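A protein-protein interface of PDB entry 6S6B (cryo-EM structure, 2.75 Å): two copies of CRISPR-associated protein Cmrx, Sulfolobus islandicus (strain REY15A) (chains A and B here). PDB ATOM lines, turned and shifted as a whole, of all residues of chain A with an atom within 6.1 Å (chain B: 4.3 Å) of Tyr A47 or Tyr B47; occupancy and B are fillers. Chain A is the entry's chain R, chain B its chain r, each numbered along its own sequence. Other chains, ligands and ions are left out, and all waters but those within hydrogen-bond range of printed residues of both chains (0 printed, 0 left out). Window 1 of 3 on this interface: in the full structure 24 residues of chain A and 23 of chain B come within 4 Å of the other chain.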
ATOM      1  N   ILE A  44      11.332  14.863 -19.056  1.00  0.00           N
ATOM      2  CA  ILE A  44      11.115  16.196 -18.510  1.00  0.00           C
ATOM      3  C   ILE A  44      12.433  16.684 -17.928  1.00  0.00           C
ATOM      4  O   ILE A  44      13.118  15.939 -17.217  1.00  0.00           O
ATOM      5  CB  ILE A  44       9.999  16.199 -17.453  1.00  0.00           C
ATOM      6  CG1 ILE A  44       8.671  15.797 -18.087  1.00  0.00           C
ATOM      7  CG2 ILE A  44       9.862  17.562 -16.821  1.00  0.00           C
ATOM      8  CD1 ILE A  44       7.541  15.710 -17.105  1.00  0.00           C
ATOM      9  N   THR A  45      12.789  17.927 -18.233  1.00  0.00           N
ATOM     10  CA  THR A  45      14.068  18.492 -17.839  1.00  0.00           C
ATOM     11  C   THR A  45      13.885  19.510 -16.721  1.00  0.00           C
ATOM     12  O   THR A  45      12.858  20.188 -16.638  1.00  0.00           O
ATOM     13  CB  THR A  45      14.763  19.152 -19.029  1.00  0.00           C
ATOM     14  OG1 THR A  45      13.990  20.274 -19.475  1.00  0.00           O
ATOM     15  CG2 THR A  45      14.901  18.158 -20.167  1.00  0.00           C
ATOM     16  N   GLY A  46      14.897  19.611 -15.864  1.00  0.00           N
ATOM     17  CA  GLY A  46      14.855  20.556 -14.766  1.00  0.00           C
ATOM     18  C   GLY A  46      14.135  20.068 -13.529  1.00  0.00           C
ATOM     19  O   GLY A  46      13.562  20.880 -12.795  1.00  0.00           O
ATOM     20  N   TYR A  47      14.142  18.762 -13.273  1.00  0.00           N
ATOM     21  CA  TYR A  47      13.451  18.202 -12.123  1.00  0.00           C
ATOM     22  C   TYR A  47      14.209  16.980 -11.629  1.00  0.00           C
ATOM     23  O   TYR A  47      14.872  16.288 -12.404  1.00  0.00           O
ATOM     24  CB  TYR A  47      12.008  17.820 -12.464  1.00  0.00           C
ATOM     25  CG  TYR A  47      11.145  18.979 -12.894  1.00  0.00           C
ATOM     26  CD1 TYR A  47      11.104  19.382 -14.218  1.00  0.00           C
ATOM     27  CD2 TYR A  47      10.363  19.664 -11.977  1.00  0.00           C
ATOM     28  CE1 TYR A  47      10.322  20.438 -14.617  1.00  0.00           C
ATOM     29  CE2 TYR A  47       9.574  20.723 -12.368  1.00  0.00           C
ATOM     30  CZ  TYR A  47       9.559  21.105 -13.689  1.00  0.00           C
ATOM     31  OH  TYR A  47       8.773  22.160 -14.084  1.00  0.00           O
ATOM     32  N   ALA A  48      14.094  16.717 -10.329  1.00  0.00           N
ATOM     33  CA  ALA A  48      14.714  15.562  -9.700  1.00  0.00           C
ATOM     34  C   ALA A  48      13.676  14.846  -8.843  1.00  0.00           C
ATOM     35  O   ALA A  48      12.602  15.381  -8.564  1.00  0.00           O
ATOM     36  CB  ALA A  48      15.929  15.966  -8.859  1.00  0.00           C
ATOM     37  N   VAL A  49      14.008  13.621  -8.419  1.00  0.00           N
ATOM     38  CA  VAL A  49      13.011  12.734  -7.821  1.00  0.00           C
ATOM     39  C   VAL A  49      13.081  12.663  -6.300  1.00  0.00           C
ATOM     40  O   VAL A  49      12.128  12.163  -5.678  1.00  0.00           O
ATOM     41  CB  VAL A  49      13.117  11.308  -8.395  1.00  0.00           C
ATOM     42  CG1 VAL A  49      13.226  11.354  -9.907  1.00  0.00           C
ATOM     43  CG2 VAL A  49      14.293  10.581  -7.775  1.00  0.00           C
ATOM     44  N   LEU A  56       8.580  15.778  -8.475  1.00  0.00           N
ATOM     45  CA  LEU A  56       9.554  16.515  -9.269  1.00  0.00           C
ATOM     46  C   LEU A  56       9.645  17.946  -8.762  1.00  0.00           C
ATOM     47  O   LEU A  56       8.779  18.774  -9.062  1.00  0.00           O
ATOM     48  CB  LEU A  56       9.167  16.479 -10.744  1.00  0.00           C
ATOM     49  CG  LEU A  56       8.841  15.082 -11.271  1.00  0.00           C
ATOM     50  CD1 LEU A  56       8.636  15.119 -12.770  1.00  0.00           C
ATOM     51  CD2 LEU A  56       9.931  14.090 -10.895  1.00  0.00           C
ATOM     52  N   VAL A  57      10.694  18.236  -8.001  1.00  0.00           N
ATOM     53  CA  VAL A  57      10.960  19.594  -7.543  1.00  0.00           C
ATOM     54  C   VAL A  57      11.646  20.357  -8.668  1.00  0.00           C
ATOM     55  O   VAL A  57      12.619  19.860  -9.253  1.00  0.00           O
ATOM     56  CB  VAL A  57      11.801  19.596  -6.261  1.00  0.00           C
ATOM     57  CG1 VAL A  57      12.987  18.693  -6.425  1.00  0.00           C
ATOM     58  CG2 VAL A  57      12.272  20.998  -5.952  1.00  0.00           C
ATOM     59  N   PRO A  58      11.170  21.551  -9.016  1.00  0.00           N
ATOM     60  CA  PRO A  58      11.758  22.284 -10.145  1.00  0.00           C
ATOM     61  C   PRO A  58      13.148  22.799  -9.807  1.00  0.00           C
ATOM     62  O   PRO A  58      13.324  23.602  -8.889  1.00  0.00           O
ATOM     63  CB  PRO A  58      10.769  23.433 -10.377  1.00  0.00           C
ATOM     64  CG  PRO A  58      10.033  23.572  -9.103  1.00  0.00           C
ATOM     65  CD  PRO A  58       9.969  22.213  -8.488  1.00  0.00           C
ATOM     66  N   THR A  59      14.136  22.317 -10.548  1.00  0.00           N
ATOM     67  CA  THR A  59      15.469  22.893 -10.523  1.00  0.00           C
ATOM     68  C   THR A  59      15.549  23.954 -11.615  1.00  0.00           C
ATOM     69  O   THR A  59      14.535  24.368 -12.183  1.00  0.00           O
ATOM     70  CB  THR A  59      16.526  21.808 -10.697  1.00  0.00           C
ATOM     71  OG1 THR A  59      16.553  21.383 -12.064  1.00  0.00           O
ATOM     72  CG2 THR A  59      16.206  20.611  -9.814  1.00  0.00           C
ATOM     73  N   LEU A  60      16.756  24.410 -11.924  1.00  0.00           N
ATOM     74  CA  LEU A  60      16.949  25.427 -12.947  1.00  0.00           C
ATOM     75  C   LEU A  60      17.856  24.995 -14.089  1.00  0.00           C
ATOM     76  O   LEU A  60      17.645  25.436 -15.219  1.00  0.00           O
ATOM     77  CB  LEU A  60      17.515  26.705 -12.316  1.00  0.00           C
ATOM     78  CG  LEU A  60      16.551  27.391 -11.353  1.00  0.00           C
ATOM     79  CD1 LEU A  60      17.130  28.703 -10.856  1.00  0.00           C
ATOM     80  CD2 LEU A  60      15.212  27.606 -12.030  1.00  0.00           C
ATOM     81  N   ASP A  61      18.847  24.148 -13.827  1.00  0.00           N
ATOM     82  CA  ASP A  61      19.787  23.687 -14.833  1.00  0.00           C
ATOM     83  C   ASP A  61      19.110  22.738 -15.815  1.00  0.00           C
ATOM     84  O   ASP A  61      18.262  21.931 -15.427  1.00  0.00           O
ATOM     85  CB  ASP A  61      20.958  22.977 -14.175  1.00  0.00           C
ATOM     86  CG  ASP A  61      20.513  21.839 -13.288  1.00  0.00           C
ATOM     87  OD1 ASP A  61      19.433  21.966 -12.676  1.00  0.00           O
ATOM     88  OD2 ASP A  61      21.230  20.820 -13.213  1.00  0.00           O
ATOM     89  N   ASP A  64      18.984  18.149 -15.601  1.00  0.00           N
ATOM     90  CA  ASP A  64      18.310  17.205 -14.728  1.00  0.00           C
ATOM     91  C   ASP A  64      17.156  16.555 -15.475  1.00  0.00           C
ATOM     92  O   ASP A  64      16.278  17.246 -15.995  1.00  0.00           O
ATOM     93  CB  ASP A  64      17.814  17.903 -13.469  1.00  0.00           C
ATOM     94  CG  ASP A  64      18.936  18.253 -12.520  1.00  0.00           C
ATOM     95  OD1 ASP A  64      19.852  17.426 -12.354  1.00  0.00           O
ATOM     96  OD2 ASP A  64      18.896  19.358 -11.942  1.00  0.00           O
ATOM     97  N   TYR A  65      17.161  15.231 -15.522  1.00  0.00           N
ATOM     98  CA  TYR A  65      16.180  14.472 -16.274  1.00  0.00           C
ATOM     99  C   TYR A  65      15.267  13.694 -15.342  1.00  0.00           C
ATOM    100  O   TYR A  65      15.674  13.266 -14.260  1.00  0.00           O
ATOM    101  CB  TYR A  65      16.858  13.493 -17.232  1.00  0.00           C
ATOM    102  CG  TYR A  65      17.662  14.174 -18.292  1.00  0.00           C
ATOM    103  CD1 TYR A  65      17.157  15.279 -18.958  1.00  0.00           C
ATOM    104  CD2 TYR A  65      18.920  13.713 -18.641  1.00  0.00           C
ATOM    105  CE1 TYR A  65      17.885  15.915 -19.938  1.00  0.00           C
ATOM    106  CE2 TYR A  65      19.660  14.342 -19.624  1.00  0.00           C
ATOM    107  CZ  TYR A  65      19.134  15.443 -20.270  1.00  0.00           C
ATOM    108  OH  TYR A  65      19.856  16.077 -21.249  1.00  0.00           O
ATOM    109  N   VAL A  66      14.022  13.526 -15.774  1.00  0.00           N
ATOM    110  CA  VAL A  66      13.137  12.521 -15.198  1.00  0.00           C
ATOM    111  C   VAL A  66      12.455  11.785 -16.344  1.00  0.00           C
ATOM    112  O   VAL A  66      11.416  12.212 -16.858  1.00  0.00           O
ATOM    113  CB  VAL A  66      12.138  13.143 -14.201  1.00  0.00           C
ATOM    114  CG1 VAL A  66      12.861  13.629 -12.961  1.00  0.00           C
ATOM    115  CG2 VAL A  66      11.429  14.328 -14.817  1.00  0.00           C
ATOM    116  N   LEU A  84       0.822  18.859 -11.272  1.00  0.00           N
ATOM    117  CA  LEU A  84       0.911  20.086 -12.054  1.00  0.00           C
ATOM    118  C   LEU A  84      -0.433  20.486 -12.643  1.00  0.00           C
ATOM    119  O   LEU A  84      -0.787  21.671 -12.641  1.00  0.00           O
ATOM    120  CB  LEU A  84       1.944  19.925 -13.164  1.00  0.00           C
ATOM    121  CG  LEU A  84       3.384  20.203 -12.753  1.00  0.00           C
ATOM    122  CD1 LEU A  84       4.285  20.207 -13.968  1.00  0.00           C
ATOM    123  CD2 LEU A  84       3.468  21.526 -12.017  1.00  0.00           C
ATOM    124  N   TYR A 112       4.461  16.983  -9.018  1.00  0.00           N
ATOM    125  CA  TYR A 112       5.201  18.198  -8.708  1.00  0.00           C
ATOM    126  C   TYR A 112       5.315  18.385  -7.201  1.00  0.00           C
ATOM    127  O   TYR A 112       4.320  18.279  -6.478  1.00  0.00           O
ATOM    128  CB  TYR A 112       4.519  19.413  -9.339  1.00  0.00           C
ATOM    129  CG  TYR A 112       5.097  20.753  -8.935  1.00  0.00           C
ATOM    130  CD1 TYR A 112       4.636  21.422  -7.808  1.00  0.00           C
ATOM    131  CD2 TYR A 112       6.092  21.357  -9.689  1.00  0.00           C
ATOM    132  CE1 TYR A 112       5.157  22.642  -7.441  1.00  0.00           C
ATOM    133  CE2 TYR A 112       6.617  22.578  -9.330  1.00  0.00           C
ATOM    134  CZ  TYR A 112       6.148  23.216  -8.204  1.00  0.00           C
ATOM    135  OH  TYR A 112       6.670  24.436  -7.840  1.00  0.00           O
ATOM    136  N   THR A 123      21.882  17.904  -7.291  1.00  0.00           N
ATOM    137  CA  THR A 123      21.313  16.711  -7.893  1.00  0.00           C
ATOM    138  C   THR A 123      22.366  15.622  -8.044  1.00  0.00           C
ATOM    139  O   THR A 123      23.558  15.892  -8.215  1.00  0.00           O
ATOM    140  CB  THR A 123      20.704  17.032  -9.256  1.00  0.00           C
ATOM    141  OG1 THR A 123      21.692  17.652 -10.088  1.00  0.00           O
ATOM    142  CG2 THR A 123      19.530  17.974  -9.090  1.00  0.00           C
ATOM    143  N   TYR A 170      17.977  12.082 -12.193  1.00  0.00           N
ATOM    144  CA  TYR A 170      18.705  12.725 -11.113  1.00  0.00           C
ATOM    145  C   TYR A 170      17.846  12.706  -9.857  1.00  0.00           C
ATOM    146  O   TYR A 170      16.628  12.523  -9.914  1.00  0.00           O
ATOM    147  CB  TYR A 170      19.079  14.169 -11.459  1.00  0.00           C
ATOM    148  CG  TYR A 170      20.137  14.290 -12.524  1.00  0.00           C
ATOM    149  CD1 TYR A 170      19.836  14.050 -13.854  1.00  0.00           C
ATOM    150  CD2 TYR A 170      21.435  14.653 -12.201  1.00  0.00           C
ATOM    151  CE1 TYR A 170      20.796  14.159 -14.827  1.00  0.00           C
ATOM    152  CE2 TYR A 170      22.403  14.770 -13.173  1.00  0.00           C
ATOM    153  CZ  TYR A 170      22.078  14.522 -14.485  1.00  0.00           C
ATOM    154  OH  TYR A 170      23.040  14.635 -15.461  1.00  0.00           O
ATOM    155  N   ILE B  44      16.474  30.501 -17.850  1.00  0.00           N
ATOM    156  CA  ILE B  44      15.582  29.453 -17.378  1.00  0.00           C
ATOM    157  C   ILE B  44      15.006  28.756 -18.600  1.00  0.00           C
ATOM    158  O   ILE B  44      14.755  29.389 -19.629  1.00  0.00           O
ATOM    159  CB  ILE B  44      14.463  30.029 -16.487  1.00  0.00           C
ATOM    160  CG1 ILE B  44      15.049  30.977 -15.444  1.00  0.00           C
ATOM    161  CG2 ILE B  44      13.709  28.919 -15.787  1.00  0.00           C
ATOM    162  CD1 ILE B  44      16.022  30.312 -14.510  1.00  0.00           C
ATOM    163  N   THR B  45      14.795  27.449 -18.492  1.00  0.00           N
ATOM    164  CA  THR B  45      14.293  26.671 -19.612  1.00  0.00           C
ATOM    165  C   THR B  45      13.054  25.895 -19.189  1.00  0.00           C
ATOM    166  O   THR B  45      12.917  25.493 -18.032  1.00  0.00           O
ATOM    167  CB  THR B  45      15.364  25.712 -20.167  1.00  0.00           C
ATOM    168  OG1 THR B  45      14.940  25.197 -21.434  1.00  0.00           O
ATOM    169  CG2 THR B  45      15.616  24.558 -19.213  1.00  0.00           C
ATOM    170  N   GLY B  46      12.144  25.705 -20.141  1.00  0.00           N
ATOM    171  CA  GLY B  46      10.876  25.075 -19.845  1.00  0.00           C
ATOM    172  C   GLY B  46       9.871  25.988 -19.180  1.00  0.00           C
ATOM    173  O   GLY B  46       9.063  25.522 -18.373  1.00  0.00           O
ATOM    174  N   TYR B  47       9.903  27.281 -19.491  1.00  0.00           N
ATOM    175  CA  TYR B  47       9.033  28.265 -18.864  1.00  0.00           C
ATOM    176  C   TYR B  47       8.737  29.365 -19.872  1.00  0.00           C
ATOM    177  O   TYR B  47       9.583  29.703 -20.702  1.00  0.00           O
ATOM    178  CB  TYR B  47       9.675  28.874 -17.611  1.00  0.00           C
ATOM    179  CG  TYR B  47       9.826  27.927 -16.441  1.00  0.00           C
ATOM    180  CD1 TYR B  47      10.881  27.031 -16.379  1.00  0.00           C
ATOM    181  CD2 TYR B  47       8.928  27.948 -15.385  1.00  0.00           C
ATOM    182  CE1 TYR B  47      11.026  26.171 -15.315  1.00  0.00           C
ATOM    183  CE2 TYR B  47       9.066  27.092 -14.315  1.00  0.00           C
ATOM    184  CZ  TYR B  47      10.117  26.205 -14.285  1.00  0.00           C
ATOM    185  OH  TYR B  47      10.261  25.349 -13.220  1.00  0.00           O
ATOM    186  N   ALA B  48       7.531  29.922 -19.793  1.00  0.00           N
ATOM    187  CA  ALA B  48       7.132  31.040 -20.636  1.00  0.00           C
ATOM    188  C   ALA B  48       6.517  32.128 -19.770  1.00  0.00           C
ATOM    189  O   ALA B  48       5.740  31.838 -18.857  1.00  0.00           O
ATOM    190  CB  ALA B  48       6.140  30.601 -21.715  1.00  0.00           C
ATOM    191  N   LEU B  56       6.158  33.360 -15.564  1.00  0.00           N
ATOM    192  CA  LEU B  56       6.879  32.160 -15.985  1.00  0.00           C
ATOM    193  C   LEU B  56       6.066  30.894 -15.726  1.00  0.00           C
ATOM    194  O   LEU B  56       6.431  30.046 -14.912  1.00  0.00           O
ATOM    195  CB  LEU B  56       8.237  32.074 -15.292  1.00  0.00           C
ATOM    196  CG  LEU B  56       9.101  33.323 -15.397  1.00  0.00           C
ATOM    197  CD1 LEU B  56      10.409  33.070 -14.712  1.00  0.00           C
ATOM    198  CD2 LEU B  56       9.316  33.707 -16.842  1.00  0.00           C
ATOM    199  N   VAL B  57       4.943  30.789 -16.424  1.00  0.00           N
ATOM    200  CA  VAL B  57       4.106  29.597 -16.343  1.00  0.00           C
ATOM    201  C   VAL B  57       4.959  28.388 -16.708  1.00  0.00           C
ATOM    202  O   VAL B  57       5.567  28.361 -17.788  1.00  0.00           O
ATOM    203  CB  VAL B  57       2.876  29.712 -17.253  1.00  0.00           C
ATOM    204  CG1 VAL B  57       2.255  28.353 -17.462  1.00  0.00           C
ATOM    205  CG2 VAL B  57       1.862  30.669 -16.650  1.00  0.00           C
ATOM    206  N   PRO B  58       5.043  27.380 -15.845  1.00  0.00           N
ATOM    207  CA  PRO B  58       5.973  26.272 -16.096  1.00  0.00           C
ATOM    208  C   PRO B  58       5.523  25.356 -17.220  1.00  0.00           C
ATOM    209  O   PRO B  58       4.576  24.582 -17.064  1.00  0.00           O
ATOM    210  CB  PRO B  58       5.999  25.535 -14.753  1.00  0.00           C
ATOM    211  CG  PRO B  58       4.675  25.820 -14.154  1.00  0.00           C
ATOM    212  CD  PRO B  58       4.318  27.216 -14.577  1.00  0.00           C
ATOM    213  N   THR B  59       6.199  25.436 -18.359  1.00  0.00           N
ATOM    214  CA  THR B  59       5.951  24.516 -19.452  1.00  0.00           C
ATOM    215  C   THR B  59       6.829  23.279 -19.258  1.00  0.00           C
ATOM    216  O   THR B  59       7.609  23.185 -18.308  1.00  0.00           O
ATOM    217  CB  THR B  59       6.218  25.203 -20.793  1.00  0.00           C
ATOM    218  OG1 THR B  59       5.775  26.562 -20.722  1.00  0.00           O
ATOM    219  CG2 THR B  59       5.451  24.518 -21.916  1.00  0.00           C
ATOM    220  N   ASP B  64      11.351  26.049 -24.803  1.00  0.00           N
ATOM    221  CA  ASP B  64      10.869  27.317 -24.274  1.00  0.00           C
ATOM    222  C   ASP B  64      11.812  27.798 -23.185  1.00  0.00           C
ATOM    223  O   ASP B  64      12.104  27.061 -22.240  1.00  0.00           O
ATOM    224  CB  ASP B  64       9.454  27.192 -23.715  1.00  0.00           C
ATOM    225  CG  ASP B  64       8.477  26.669 -24.731  1.00  0.00           C
ATOM    226  OD1 ASP B  64       8.223  27.376 -25.723  1.00  0.00           O
ATOM    227  OD2 ASP B  64       7.934  25.568 -24.527  1.00  0.00           O
ATOM    228  N   TYR B  65      12.281  29.032 -23.318  1.00  0.00           N
ATOM    229  CA  TYR B  65      13.225  29.593 -22.369  1.00  0.00           C
ATOM    230  C   TYR B  65      12.850  31.034 -22.080  1.00  0.00           C
ATOM    231  O   TYR B  65      12.132  31.679 -22.846  1.00  0.00           O
ATOM    232  CB  TYR B  65      14.663  29.521 -22.892  1.00  0.00           C
ATOM    233  CG  TYR B  65      14.882  30.311 -24.157  1.00  0.00           C
ATOM    234  CD1 TYR B  65      14.582  29.766 -25.397  1.00  0.00           C
ATOM    235  CD2 TYR B  65      15.382  31.602 -24.114  1.00  0.00           C
ATOM    236  CE1 TYR B  65      14.776  30.484 -26.551  1.00  0.00           C
ATOM    237  CE2 TYR B  65      15.579  32.326 -25.265  1.00  0.00           C
ATOM    238  CZ  TYR B  65      15.274  31.763 -26.480  1.00  0.00           C
ATOM    239  OH  TYR B  65      15.470  32.483 -27.634  1.00  0.00           O
ATOM    240  N   VAL B  66      13.345  31.530 -20.952  1.00  0.00           N
ATOM    241  CA  VAL B  66      13.187  32.923 -20.558  1.00  0.00           C
ATOM    242  C   VAL B  66      14.504  33.382 -19.958  1.00  0.00           C
ATOM    243  O   VAL B  66      15.033  32.738 -19.048  1.00  0.00           O
ATOM    244  CB  VAL B  66      12.047  33.123 -19.543  1.00  0.00           C
ATOM    245  CG1 VAL B  66      11.986  34.569 -19.116  1.00  0.00           C
ATOM    246  CG2 VAL B  66      10.720  32.695 -20.130  1.00  0.00           C
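The backbone carbonyl oxygen of Ile B44 lies within hydrogen-bond range of the backbone NH of Val B66.
Tyr A47 touches Tyr B47. Tyr B47 touches Pro A58 (OH to CB, 3.5 Å). CD1 of Ile B44 touches CD2 of Leu A60, 3.8 Å away.
Of chain B, only Tyr B47 (3.6 Å) comes within 4 Å of Tyr A47. Of chain A, only Tyr A47 and Pro A58 come within 4 Å of Tyr B47. Printed residues of chain B within 4 Å of Leu A60: Ile B44 (3.8 Å). Of the printed residues of chain A, Ile B44 touches Leu A60. Of the printed residues of chain B, Pro A58 touches Tyr B47 (3.5 Å). The nearest residue of chain A that does not touch Tyr B47 is Thr A59 (4.5 Å).
Of the 12 printed residues of chain B, 2 touch a printed residue of chain A. Along chain B the printed residues that touch a printed residue of chain A span positions 44 to 47. Of the 19 printed residues of chain A, 3 touch a printed residue of chain B. Hydrophobic or aromatic side chains of chain A within 4 Å of the printed part of chain B: Tyr A47, Pro A58 and Leu A60. Among the printed residues, no Asp or Glu carboxylate lies within 4 Å of a Lys or Arg side-chain nitrogen of the other chain.
Tyr A47 touches its own counterpart, Tyr B47. Pro A58 touches Tyr B47, but with the chains exchanged Tyr A47 does not touch Pro B58 (4.4 Å). 12 positions are printed for both chains. Of the 3 pairs that touch across the chains among the printed residues, 1 has its exchanged pair printed and touching as well.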
